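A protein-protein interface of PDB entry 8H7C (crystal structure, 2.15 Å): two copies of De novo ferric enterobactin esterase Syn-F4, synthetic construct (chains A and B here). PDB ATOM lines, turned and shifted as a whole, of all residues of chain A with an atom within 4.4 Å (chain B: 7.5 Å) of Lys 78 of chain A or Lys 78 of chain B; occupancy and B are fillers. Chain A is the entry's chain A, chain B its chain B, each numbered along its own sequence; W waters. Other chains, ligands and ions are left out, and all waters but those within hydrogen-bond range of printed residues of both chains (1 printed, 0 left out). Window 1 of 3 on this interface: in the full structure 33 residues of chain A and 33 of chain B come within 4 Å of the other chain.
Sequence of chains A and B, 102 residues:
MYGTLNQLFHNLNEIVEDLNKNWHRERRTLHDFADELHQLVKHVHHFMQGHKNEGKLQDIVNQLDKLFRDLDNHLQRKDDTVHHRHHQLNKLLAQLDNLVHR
OE2 of Glu 26 of chain A is in salt-bridge range of NZ of Lys 78 of chain B (3.0 Å). A ring nitrogen (NE2) of His 74 of chain A sits at hydrogen-bond distance from the side-chain carboxylate of Glu 26 of chain B (3.0 Å). The side-chain carboxylate of Glu 26 of chain B lies within salt-bridge range of the side-chain amino group of Lys 78 of chain A (3.0 Å). OE2 of Glu 26 of chain A lies close to OE2 of Glu 26 of chain B (3.0 Å).
The side-chain amino group of Lys 78 of chain A is in salt-bridge range of the side-chain carboxylate of Glu 26 of chain A, at 3.7 Å. The backbone carbonyl oxygen of Arg 77 of chain A lies within hydrogen-bond range of the side-chain hydroxyl of Thr 81 of chain A (3.3 Å). The side-chain amino group of Lys 78 of chain B lies within salt-bridge range of the side-chain carboxylate of Glu 26 of chain B (3.1 Å).
His 74 of chain B touches Glu 26 of chain A (CE1 to CG, 3.8 Å). Leu 30 of chain B touches His 74 of chain A (CD2 to CD2, 3.9 Å). NZ of Lys 78 of chain A touches NZ of Lys 78 of chain B, at 3.7 Å. CG2 of Thr 81 of chain A touches ND2 of Asn 22 of chain B, 3.8 Å away.
Of chain B, only Glu 26 and Lys 78 come within 4 Å of Lys 78 of chain A. Lys 78 of chain B touches two residues of chain A. Of the printed residues of chain A, Glu 26 of chain B touches Glu 26, His 74 and Lys 78. Printed residues of chain A within 4 Å of Asn 22 of chain B: Thr 81. Arg 85 of chain B touches none of the printed residues of chain A. The nearest printed residue of chain A that does not touch Lys 78 of chain B is Trp 23 of chain A (6.5 Å).
Of the 11 printed residues of chain A, 4 touch a printed residue of chain B. Hydrophobic or aromatic side chains of chain A within 4 Å of the printed part of chain B: His 74. Of the 20 printed residues of chain B, 5 touch a printed residue of chain A. Hydrophobic or aromatic side chains of chain B within 4 Å of the printed part of chain A: Leu 30 and His 74. Along chain B the printed residues that touch a printed residue of chain A span positions 22 to 78. Among the printed residues, 8 pairs touch across the chains. Among the printed residues, Asp or Glu carboxylates within 4 Å of a Lys or Arg side-chain nitrogen of the other chain: Glu 26 of chain A with Lys 78 of chain B (3.0 Å) and Lys 78 of chain A with Glu 26 of chain B (3.0 Å).
Glu 26 of chain B touches its own counterpart, Glu 26 of chain A. Glu 26 of chain A touches His 74 of chain B, and with the chains exchanged His 74 of chain A touches Glu 26 of chain B. Glu 26 of chain A touches Lys 78 of chain B, and with the chains exchanged Lys 78 of chain A touches Glu 26 of chain B. Lys 78 of chain B touches its own counterpart, Lys 78 of chain A.
Water W1 bridges NH1 of Arg 85 of chain B (3.3 Å) and NZ of Lys 78 of chain A (3.4 Å).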
ATOM      1  N   TRP A  23      13.401  15.695   1.561  1.00  0.00           N
ATOM      2  CA  TRP A  23      12.591  15.190   0.452  1.00  0.00           C
ATOM      3  C   TRP A  23      12.978  13.729   0.083  1.00  0.00           C
ATOM      4  O   TRP A  23      12.121  12.830   0.007  1.00  0.00           O
ATOM      5  CB  TRP A  23      12.707  16.123  -0.762  1.00  0.00           C
ATOM      6  CG  TRP A  23      12.247  15.475  -2.002  1.00  0.00           C
ATOM      7  CD1 TRP A  23      12.957  15.308  -3.140  1.00  0.00           C
ATOM      8  CD2 TRP A  23      10.998  14.815  -2.202  1.00  0.00           C
ATOM      9  NE1 TRP A  23      12.220  14.613  -4.060  1.00  0.00           N
ATOM     10  CE2 TRP A  23      11.009  14.299  -3.501  1.00  0.00           C
ATOM     11  CE3 TRP A  23       9.864  14.608  -1.400  1.00  0.00           C
ATOM     12  CZ2 TRP A  23       9.936  13.609  -4.027  1.00  0.00           C
ATOM     13  CZ3 TRP A  23       8.794  13.925  -1.937  1.00  0.00           C
ATOM     14  CH2 TRP A  23       8.847  13.426  -3.229  1.00  0.00           C
ATOM     15  N   GLU A  26      11.695  11.437   2.852  1.00  0.00           N
ATOM     16  CA  GLU A  26      10.256  11.368   2.744  1.00  0.00           C
ATOM     17  C   GLU A  26       9.839  10.480   1.569  1.00  0.00           C
ATOM     18  O   GLU A  26       9.012   9.585   1.742  1.00  0.00           O
ATOM     19  CB  GLU A  26       9.677  12.776   2.589  1.00  0.00           C
ATOM     20  CG  GLU A  26       8.170  12.804   2.353  1.00  0.00           C
ATOM     21  CD  GLU A  26       7.598  14.216   2.240  1.00  0.00           C
ATOM     22  OE1 GLU A  26       8.377  15.189   2.123  1.00  0.00           O
ATOM     23  OE2 GLU A  26       6.345  14.337   2.260  1.00  0.00           O
ATOM     24  N   HIS A  74      -0.763  10.791  -5.410  1.00  0.00           N
ATOM     25  CA  HIS A  74      -0.067  11.741  -4.570  1.00  0.00           C
ATOM     26  C   HIS A  74       1.468  11.739  -4.807  1.00  0.00           C
ATOM     27  O   HIS A  74       2.095  12.784  -4.853  1.00  0.00           O
ATOM     28  CB  HIS A  74      -0.384  11.501  -3.107  1.00  0.00           C
ATOM     29  CG  HIS A  74       0.444  12.336  -2.203  1.00  0.00           C
ATOM     30  ND1 HIS A  74       0.333  13.707  -2.174  1.00  0.00           N
ATOM     31  CD2 HIS A  74       1.465  12.022  -1.374  1.00  0.00           C
ATOM     32  CE1 HIS A  74       1.223  14.201  -1.339  1.00  0.00           C
ATOM     33  NE2 HIS A  74       1.925  13.201  -0.844  1.00  0.00           N
ATOM     34  N   LEU A  75       2.059  10.570  -4.973  1.00  0.00           N
ATOM     35  CA  LEU A  75       3.508  10.485  -5.178  1.00  0.00           C
ATOM     36  C   LEU A  75       3.941  10.995  -6.550  1.00  0.00           C
ATOM     37  O   LEU A  75       4.963  11.686  -6.661  1.00  0.00           O
ATOM     38  CB  LEU A  75       4.032   9.058  -4.939  1.00  0.00           C
ATOM     39  CG  LEU A  75       3.824   8.480  -3.533  1.00  0.00           C
ATOM     40  CD1 LEU A  75       4.266   7.021  -3.470  1.00  0.00           C
ATOM     41  CD2 LEU A  75       4.535   9.303  -2.480  1.00  0.00           C
ATOM     42  N   GLN A  76       3.172  10.671  -7.589  1.00  0.00           N
ATOM     43  CA  GLN A  76       3.484  11.166  -8.914  1.00  0.00           C
ATOM     44  C   GLN A  76       3.346  12.684  -8.964  1.00  0.00           C
ATOM     45  O   GLN A  76       4.240  13.355  -9.440  1.00  0.00           O
ATOM     46  CB  GLN A  76       2.581  10.520  -9.963  1.00  0.00           C
ATOM     47  CG  GLN A  76       2.761   9.017 -10.105  1.00  0.00           C
ATOM     48  CD  GLN A  76       1.862   8.466 -11.192  1.00  0.00           C
ATOM     49  OE1 GLN A  76       1.998   8.846 -12.363  1.00  0.00           O
ATOM     50  NE2 GLN A  76       0.918   7.586 -10.818  1.00  0.00           N
ATOM     51  N   ARG A  77       2.242  13.210  -8.429  1.00  0.00           N
ATOM     52  CA  ARG A  77       2.031  14.660  -8.297  1.00  0.00           C
ATOM     53  C   ARG A  77       3.184  15.297  -7.540  1.00  0.00           C
ATOM     54  O   ARG A  77       3.764  16.279  -7.975  1.00  0.00           O
ATOM     55  CB  ARG A  77       0.730  14.975  -7.536  1.00  0.00           C
ATOM     56  CG  ARG A  77      -0.552  14.583  -8.250  1.00  0.00           C
ATOM     57  CD  ARG A  77      -1.101  15.677  -9.128  1.00  0.00           C
ATOM     58  NE  ARG A  77      -1.457  16.874  -8.375  1.00  0.00           N
ATOM     59  CZ  ARG A  77      -1.730  18.062  -8.924  1.00  0.00           C
ATOM     60  NH1 ARG A  77      -1.697  18.222 -10.254  1.00  0.00           N
ATOM     61  NH2 ARG A  77      -2.027  19.100  -8.143  1.00  0.00           N
ATOM     62  N   LYS A  78       3.508  14.719  -6.392  1.00  0.00           N
ATOM     63  CA  LYS A  78       4.566  15.228  -5.542  1.00  0.00           C
ATOM     64  C   LYS A  78       5.928  15.312  -6.247  1.00  0.00           C
ATOM     65  O   LYS A  78       6.604  16.312  -6.146  1.00  0.00           O
ATOM     66  CB  LYS A  78       4.635  14.352  -4.307  1.00  0.00           C
ATOM     67  CG  LYS A  78       5.759  14.673  -3.387  1.00  0.00           C
ATOM     68  CD  LYS A  78       5.594  16.027  -2.725  1.00  0.00           C
ATOM     69  CE  LYS A  78       5.614  15.831  -1.218  1.00  0.00           C
ATOM     70  NZ  LYS A  78       6.297  16.912  -0.475  1.00  0.00           N
ATOM     71  N   ASP A  79       6.322  14.270  -6.959  1.00  0.00           N
ATOM     72  CA  ASP A  79       7.555  14.327  -7.745  1.00  0.00           C
ATOM     73  C   ASP A  79       7.574  15.560  -8.650  1.00  0.00           C
ATOM     74  O   ASP A  79       8.569  16.293  -8.729  1.00  0.00           O
ATOM     75  CB  ASP A  79       7.727  13.067  -8.598  1.00  0.00           C
ATOM     76  CG  ASP A  79       8.371  11.899  -7.842  1.00  0.00           C
ATOM     77  OD1 ASP A  79       9.052  12.061  -6.797  1.00  0.00           O
ATOM     78  OD2 ASP A  79       8.188  10.772  -8.308  1.00  0.00           O
ATOM     79  N   ASP A  80       6.471  15.785  -9.340  1.00  0.00           N
ATOM     80  CA  ASP A  80       6.338  16.959 -10.224  1.00  0.00           C
ATOM     81  C   ASP A  80       6.460  18.324  -9.499  1.00  0.00           C
ATOM     82  O   ASP A  80       7.174  19.189  -9.953  1.00  0.00           O
ATOM     83  CB  ASP A  80       5.039  16.884 -11.040  1.00  0.00           C
ATOM     84  CG  ASP A  80       5.067  15.773 -12.099  1.00  0.00           C
ATOM     85  OD1 ASP A  80       6.155  15.315 -12.512  1.00  0.00           O
ATOM     86  OD2 ASP A  80       3.970  15.367 -12.530  1.00  0.00           O
ATOM     87  N   THR A  81       5.791  18.476  -8.373  1.00  0.00           N
ATOM     88  CA  THR A  81       5.889  19.685  -7.556  1.00  0.00           C
ATOM     89  C   THR A  81       7.309  19.981  -7.049  1.00  0.00           C
ATOM     90  O   THR A  81       7.779  21.111  -7.093  1.00  0.00           O
ATOM     91  CB  THR A  81       4.940  19.525  -6.378  1.00  0.00           C
ATOM     92  OG1 THR A  81       3.628  19.409  -6.919  1.00  0.00           O
ATOM     93  CG2 THR A  81       4.978  20.708  -5.425  1.00  0.00           C
ATOM     94  N   VAL A  82       7.968  18.947  -6.551  1.00  0.00           N
ATOM     95  CA  VAL A  82       9.323  19.053  -6.035  1.00  0.00           C
ATOM     96  C   VAL A  82      10.289  19.416  -7.171  1.00  0.00           C
ATOM     97  O   VAL A  82      11.218  20.187  -6.977  1.00  0.00           O
ATOM     98  CB  VAL A  82       9.747  17.717  -5.400  1.00  0.00           C
ATOM     99  CG1 VAL A  82      11.216  17.701  -5.091  1.00  0.00           C
ATOM    100  CG2 VAL A  82       8.971  17.471  -4.136  1.00  0.00           C
ATOM    101  N   LEU B  19       5.181  26.732  -1.098  1.00  0.00           N
ATOM    102  CA  LEU B  19       5.586  25.651  -0.200  1.00  0.00           C
ATOM    103  C   LEU B  19       4.560  25.390   0.890  1.00  0.00           C
ATOM    104  O   LEU B  19       4.208  24.251   1.133  1.00  0.00           O
ATOM    105  CB  LEU B  19       6.912  25.996   0.490  1.00  0.00           C
ATOM    106  CG  LEU B  19       8.172  25.466  -0.173  1.00  0.00           C
ATOM    107  CD1 LEU B  19       9.399  26.208   0.346  1.00  0.00           C
ATOM    108  CD2 LEU B  19       8.277  23.962   0.091  1.00  0.00           C
ATOM    109  N   ASN B  22       1.145  24.115  -0.497  1.00  0.00           N
ATOM    110  CA  ASN B  22       1.342  22.725  -0.892  1.00  0.00           C
ATOM    111  C   ASN B  22       1.468  21.807   0.325  1.00  0.00           C
ATOM    112  O   ASN B  22       0.960  20.691   0.318  1.00  0.00           O
ATOM    113  CB  ASN B  22       2.531  22.585  -1.869  1.00  0.00           C
ATOM    114  CG  ASN B  22       2.198  23.089  -3.282  1.00  0.00           C
ATOM    115  OD1 ASN B  22       1.097  22.903  -3.772  1.00  0.00           O
ATOM    116  ND2 ASN B  22       3.161  23.686  -3.944  1.00  0.00           N
ATOM    117  N   TRP B  23       2.102  22.295   1.386  1.00  0.00           N
ATOM    118  CA  TRP B  23       2.050  21.593   2.647  1.00  0.00           C
ATOM    119  C   TRP B  23       0.612  21.431   3.169  1.00  0.00           C
ATOM    120  O   TRP B  23       0.196  20.332   3.492  1.00  0.00           O
ATOM    121  CB  TRP B  23       2.944  22.241   3.700  1.00  0.00           C
ATOM    122  CG  TRP B  23       2.772  21.585   5.032  1.00  0.00           C
ATOM    123  CD1 TRP B  23       2.504  22.201   6.208  1.00  0.00           C
ATOM    124  CD2 TRP B  23       2.785  20.178   5.309  1.00  0.00           C
ATOM    125  NE1 TRP B  23       2.382  21.277   7.210  1.00  0.00           N
ATOM    126  CE2 TRP B  23       2.546  20.026   6.687  1.00  0.00           C
ATOM    127  CE3 TRP B  23       2.978  19.038   4.530  1.00  0.00           C
ATOM    128  CZ2 TRP B  23       2.510  18.780   7.308  1.00  0.00           C
ATOM    129  CZ3 TRP B  23       2.918  17.788   5.147  1.00  0.00           C
ATOM    130  CH2 TRP B  23       2.692  17.674   6.522  1.00  0.00           C
ATOM    131  N   GLU B  26      -1.096  18.678   1.175  1.00  0.00           N
ATOM    132  CA  GLU B  26      -0.540  17.368   1.413  1.00  0.00           C
ATOM    133  C   GLU B  26      -0.905  16.794   2.778  1.00  0.00           C
ATOM    134  O   GLU B  26      -1.214  15.613   2.869  1.00  0.00           O
ATOM    135  CB  GLU B  26       0.988  17.394   1.261  1.00  0.00           C
ATOM    136  CG  GLU B  26       1.651  16.075   1.629  1.00  0.00           C
ATOM    137  CD  GLU B  26       3.105  16.002   1.218  1.00  0.00           C
ATOM    138  OE1 GLU B  26       3.722  17.091   1.041  1.00  0.00           O
ATOM    139  OE2 GLU B  26       3.619  14.843   1.081  1.00  0.00           O
ATOM    140  N   ARG B  27      -0.822  17.617   3.818  1.00  0.00           N
ATOM    141  CA  ARG B  27      -1.215  17.219   5.173  1.00  0.00           C
ATOM    142  C   ARG B  27      -2.667  16.736   5.224  1.00  0.00           C
ATOM    143  O   ARG B  27      -2.946  15.661   5.738  1.00  0.00           O
ATOM    144  CB  ARG B  27      -1.018  18.392   6.134  1.00  0.00           C
ATOM    145  CG  ARG B  27      -1.361  18.102   7.588  1.00  0.00           C
ATOM    146  CD  ARG B  27      -0.987  19.269   8.492  1.00  0.00           C
ATOM    147  NE  ARG B  27      -0.725  18.824   9.859  1.00  0.00           N
ATOM    148  CZ  ARG B  27      -1.657  18.509  10.754  1.00  0.00           C
ATOM    149  NH1 ARG B  27      -2.943  18.579  10.456  1.00  0.00           N
ATOM    150  NH2 ARG B  27      -1.298  18.115  11.965  1.00  0.00           N
ATOM    151  N   LEU B  30      -2.932  13.496   3.224  1.00  0.00           N
ATOM    152  CA  LEU B  30      -2.356  12.377   3.987  1.00  0.00           C
ATOM    153  C   LEU B  30      -3.033  12.082   5.322  1.00  0.00           C
ATOM    154  O   LEU B  30      -3.018  10.950   5.776  1.00  0.00           O
ATOM    155  CB  LEU B  30      -0.859  12.580   4.172  1.00  0.00           C
ATOM    156  CG  LEU B  30      -0.042  12.563   2.869  1.00  0.00           C
ATOM    157  CD1 LEU B  30       1.411  12.859   3.155  1.00  0.00           C
ATOM    158  CD2 LEU B  30      -0.138  11.244   2.133  1.00  0.00           C
ATOM    159  N   ASP B  72       1.357   7.124  10.473  1.00  0.00           N
ATOM    160  CA  ASP B  72       1.168   7.944  11.664  1.00  0.00           C
ATOM    161  C   ASP B  72       2.491   8.577  12.130  1.00  0.00           C
ATOM    162  O   ASP B  72       2.582   9.808  12.263  1.00  0.00           O
ATOM    163  CB  ASP B  72       0.564   7.102  12.781  1.00  0.00           C
ATOM    164  CG  ASP B  72       0.000   7.929  13.890  1.00  0.00           C
ATOM    165  OD1 ASP B  72      -0.598   8.987  13.616  1.00  0.00           O
ATOM    166  OD2 ASP B  72       0.129   7.512  15.051  1.00  0.00           O
ATOM    167  N   ASN B  73       3.510   7.739  12.345  1.00  0.00           N
ATOM    168  CA  ASN B  73       4.857   8.216  12.706  1.00  0.00           C
ATOM    169  C   ASN B  73       5.408   9.214  11.694  1.00  0.00           C
ATOM    170  O   ASN B  73       5.938  10.238  12.078  1.00  0.00           O
ATOM    171  CB  ASN B  73       5.855   7.063  12.860  1.00  0.00           C
ATOM    172  CG  ASN B  73       7.243   7.541  13.278  1.00  0.00           C
ATOM    173  OD1 ASN B  73       7.427   8.019  14.397  1.00  0.00           O
ATOM    174  ND2 ASN B  73       8.219   7.445  12.371  1.00  0.00           N
ATOM    175  N   HIS B  74       5.246   8.916  10.407  1.00  0.00           N
ATOM    176  CA  HIS B  74       5.748   9.786   9.366  1.00  0.00           C
ATOM    177  C   HIS B  74       5.110  11.182   9.377  1.00  0.00           C
ATOM    178  O   HIS B  74       5.800  12.201   9.201  1.00  0.00           O
ATOM    179  CB  HIS B  74       5.575   9.159   7.990  1.00  0.00           C
ATOM    180  CG  HIS B  74       5.811  10.137   6.891  1.00  0.00           C
ATOM    181  ND1 HIS B  74       7.043  10.715   6.676  1.00  0.00           N
ATOM    182  CD2 HIS B  74       4.958  10.731   6.030  1.00  0.00           C
ATOM    183  CE1 HIS B  74       6.950  11.590   5.697  1.00  0.00           C
ATOM    184  NE2 HIS B  74       5.696  11.618   5.286  1.00  0.00           N
ATOM    185  N   LEU B  75       3.801  11.230   9.584  1.00  0.00           N
ATOM    186  CA  LEU B  75       3.086  12.506   9.606  1.00  0.00           C
ATOM    187  C   LEU B  75       3.415  13.358  10.829  1.00  0.00           C
ATOM    188  O   LEU B  75       3.550  14.563  10.722  1.00  0.00           O
ATOM    189  CB  LEU B  75       1.581  12.267   9.496  1.00  0.00           C
ATOM    190  CG  LEU B  75       1.146  11.580   8.204  1.00  0.00           C
ATOM    191  CD1 LEU B  75      -0.335  11.300   8.307  1.00  0.00           C
ATOM    192  CD2 LEU B  75       1.453  12.390   6.956  1.00  0.00           C
ATOM    193  N   GLN B  76       3.549  12.725  11.986  1.00  0.00           N
ATOM    194  CA  GLN B  76       4.043  13.401  13.196  1.00  0.00           C
ATOM    195  C   GLN B  76       5.405  14.086  12.971  1.00  0.00           C
ATOM    196  O   GLN B  76       5.598  15.249  13.323  1.00  0.00           O
ATOM    197  CB  GLN B  76       4.137  12.387  14.346  1.00  0.00           C
ATOM    198  CG  GLN B  76       2.772  11.982  14.870  1.00  0.00           C
ATOM    199  CD  GLN B  76       2.843  11.070  16.075  1.00  0.00           C
ATOM    200  OE1 GLN B  76       2.450   9.908  15.997  1.00  0.00           O
ATOM    201  NE2 GLN B  76       3.337  11.592  17.206  1.00  0.00           N
ATOM    202  N   ARG B  77       6.331  13.333  12.387  1.00  0.00           N
ATOM    203  CA  ARG B  77       7.673  13.838  12.086  1.00  0.00           C
ATOM    204  C   ARG B  77       7.696  14.911  11.018  1.00  0.00           C
ATOM    205  O   ARG B  77       8.477  15.866  11.130  1.00  0.00           O
ATOM    206  CB  ARG B  77       8.626  12.701  11.713  1.00  0.00           C
ATOM    207  CG  ARG B  77       9.136  11.988  12.951  1.00  0.00           C
ATOM    208  CD  ARG B  77      10.239  11.006  12.646  1.00  0.00           C
ATOM    209  NE  ARG B  77      11.446  11.622  12.075  1.00  0.00           N
ATOM    210  CZ  ARG B  77      12.372  12.310  12.757  1.00  0.00           C
ATOM    211  NH1 ARG B  77      12.251  12.526  14.072  1.00  0.00           N
ATOM    212  NH2 ARG B  77      13.433  12.800  12.103  1.00  0.00           N
ATOM    213  N   LYS B  78       6.854  14.775   9.997  1.00  0.00           N
ATOM    214  CA  LYS B  78       6.788  15.804   8.979  1.00  0.00           C
ATOM    215  C   LYS B  78       6.272  17.120   9.552  1.00  0.00           C
ATOM    216  O   LYS B  78       6.809  18.167   9.249  1.00  0.00           O
ATOM    217  CB  LYS B  78       5.944  15.400   7.775  1.00  0.00           C
ATOM    218  CG  LYS B  78       6.039  16.483   6.722  1.00  0.00           C
ATOM    219  CD  LYS B  78       6.088  16.005   5.299  1.00  0.00           C
ATOM    220  CE  LYS B  78       6.673  17.099   4.423  1.00  0.00           C
ATOM    221  NZ  LYS B  78       5.932  17.133   3.157  1.00  0.00           N
ATOM    222  N   ASP B  79       5.238  17.056  10.378  1.00  0.00           N
ATOM    223  CA  ASP B  79       4.754  18.224  11.092  1.00  0.00           C
ATOM    224  C   ASP B  79       5.893  18.955  11.764  1.00  0.00           C
ATOM    225  O   ASP B  79       6.029  20.151  11.606  1.00  0.00           O
ATOM    226  CB  ASP B  79       3.720  17.830  12.144  1.00  0.00           C
ATOM    227  CG  ASP B  79       2.309  17.952  11.661  1.00  0.00           C
ATOM    228  OD1 ASP B  79       2.067  18.195  10.457  1.00  0.00           O
ATOM    229  OD2 ASP B  79       1.419  17.795  12.514  1.00  0.00           O
ATOM    230  N   ASP B  80       6.711  18.221  12.501  1.00  0.00           N
ATOM    231  CA  ASP B  80       7.864  18.798  13.159  1.00  0.00           C
ATOM    232  C   ASP B  80       8.811  19.446  12.148  1.00  0.00           C
ATOM    233  O   ASP B  80       9.202  20.591  12.323  1.00  0.00           O
ATOM    234  CB  ASP B  80       8.620  17.734  13.967  1.00  0.00           C
ATOM    235  CG  ASP B  80       7.858  17.266  15.197  1.00  0.00           C
ATOM    236  OD1 ASP B  80       6.841  17.900  15.580  1.00  0.00           O
ATOM    237  OD2 ASP B  80       8.317  16.270  15.803  1.00  0.00           O
ATOM    238  N   THR B  81       9.160  18.708  11.094  1.00  0.00           N
ATOM    239  CA  THR B  81      10.136  19.179  10.109  1.00  0.00           C
ATOM    240  C   THR B  81       9.640  20.413   9.356  1.00  0.00           C
ATOM    241  O   THR B  81      10.382  21.366   9.139  1.00  0.00           O
ATOM    242  CB  THR B  81      10.450  18.094   9.084  1.00  0.00           C
ATOM    243  OG1 THR B  81      10.932  16.931   9.756  1.00  0.00           O
ATOM    244  CG2 THR B  81      11.509  18.593   8.107  1.00  0.00           C
ATOM    245  N   VAL B  82       8.379  20.380   8.961  1.00  0.00           N
ATOM    246  CA  VAL B  82       7.749  21.512   8.289  1.00  0.00           C
ATOM    247  C   VAL B  82       7.687  22.729   9.205  1.00  0.00           C
ATOM    248  O   VAL B  82       8.032  23.819   8.760  1.00  0.00           O
ATOM    249  CB  VAL B  82       6.340  21.200   7.792  1.00  0.00           C
ATOM    250  CG1 VAL B  82       5.771  22.407   7.057  1.00  0.00           C
ATOM    251  CG2 VAL B  82       6.366  20.048   6.811  1.00  0.00           C
ATOM    252  N   HIS B  83       7.280  22.535  10.468  1.00  0.00           N
ATOM    253  CA  HIS B  83       7.185  23.636  11.447  1.00  0.00           C
ATOM    254  C   HIS B  83       8.513  24.376  11.475  1.00  0.00           C
ATOM    255  O   HIS B  83       8.556  25.578  11.275  1.00  0.00           O
ATOM    256  CB  HIS B  83       6.779  23.120  12.842  1.00  0.00           C
ATOM    257  CG  HIS B  83       6.887  24.139  13.943  1.00  0.00           C
ATOM    258  ND1 HIS B  83       5.787  24.739  14.518  1.00  0.00           N
ATOM    259  CD2 HIS B  83       7.967  24.633  14.599  1.00  0.00           C
ATOM    260  CE1 HIS B  83       6.184  25.572  15.464  1.00  0.00           C
ATOM    261  NE2 HIS B  83       7.504  25.528  15.531  1.00  0.00           N
ATOM    262  N   HIS B  84       9.591  23.628  11.652  1.00  0.00           N
ATOM    263  CA  HIS B  84      10.932  24.185  11.727  1.00  0.00           C
ATOM    264  C   HIS B  84      11.396  24.897  10.444  1.00  0.00           C
ATOM    265  O   HIS B  84      11.984  25.979  10.490  1.00  0.00           O
ATOM    266  CB  HIS B  84      11.920  23.075  12.113  1.00  0.00           C
ATOM    267  CG  HIS B  84      13.333  23.554  12.251  1.00  0.00           C
ATOM    268  ND1 HIS B  84      14.371  23.032  11.510  1.00  0.00           N
ATOM    269  CD2 HIS B  84      13.872  24.524  13.023  1.00  0.00           C
ATOM    270  CE1 HIS B  84      15.492  23.651  11.832  1.00  0.00           C
ATOM    271  NE2 HIS B  84      15.213  24.567  12.741  1.00  0.00           N
ATOM    272  N   ARG B  85      11.141  24.281   9.296  1.00  0.00           N
ATOM    273  CA  ARG B  85      11.542  24.875   8.018  1.00  0.00           C
ATOM    274  C   ARG B  85      10.708  26.122   7.697  1.00  0.00           C
ATOM    275  O   ARG B  85      11.228  27.088   7.143  1.00  0.00           O
ATOM    276  CB  ARG B  85      11.464  23.829   6.906  1.00  0.00           C
ATOM    277  CG  ARG B  85      10.909  24.288   5.571  1.00  0.00           C
ATOM    278  CD  ARG B  85      10.243  23.110   4.861  1.00  0.00           C
ATOM    279  NE  ARG B  85       8.855  23.324   4.446  1.00  0.00           N
ATOM    280  CZ  ARG B  85       8.127  22.412   3.799  1.00  0.00           C
ATOM    281  NH1 ARG B  85       8.651  21.220   3.496  1.00  0.00           N
ATOM    282  NH2 ARG B  85       6.871  22.683   3.461  1.00  0.00           N
HETATM  283  O   HOH W   1       6.912  19.839   1.042  1.00  0.00           O
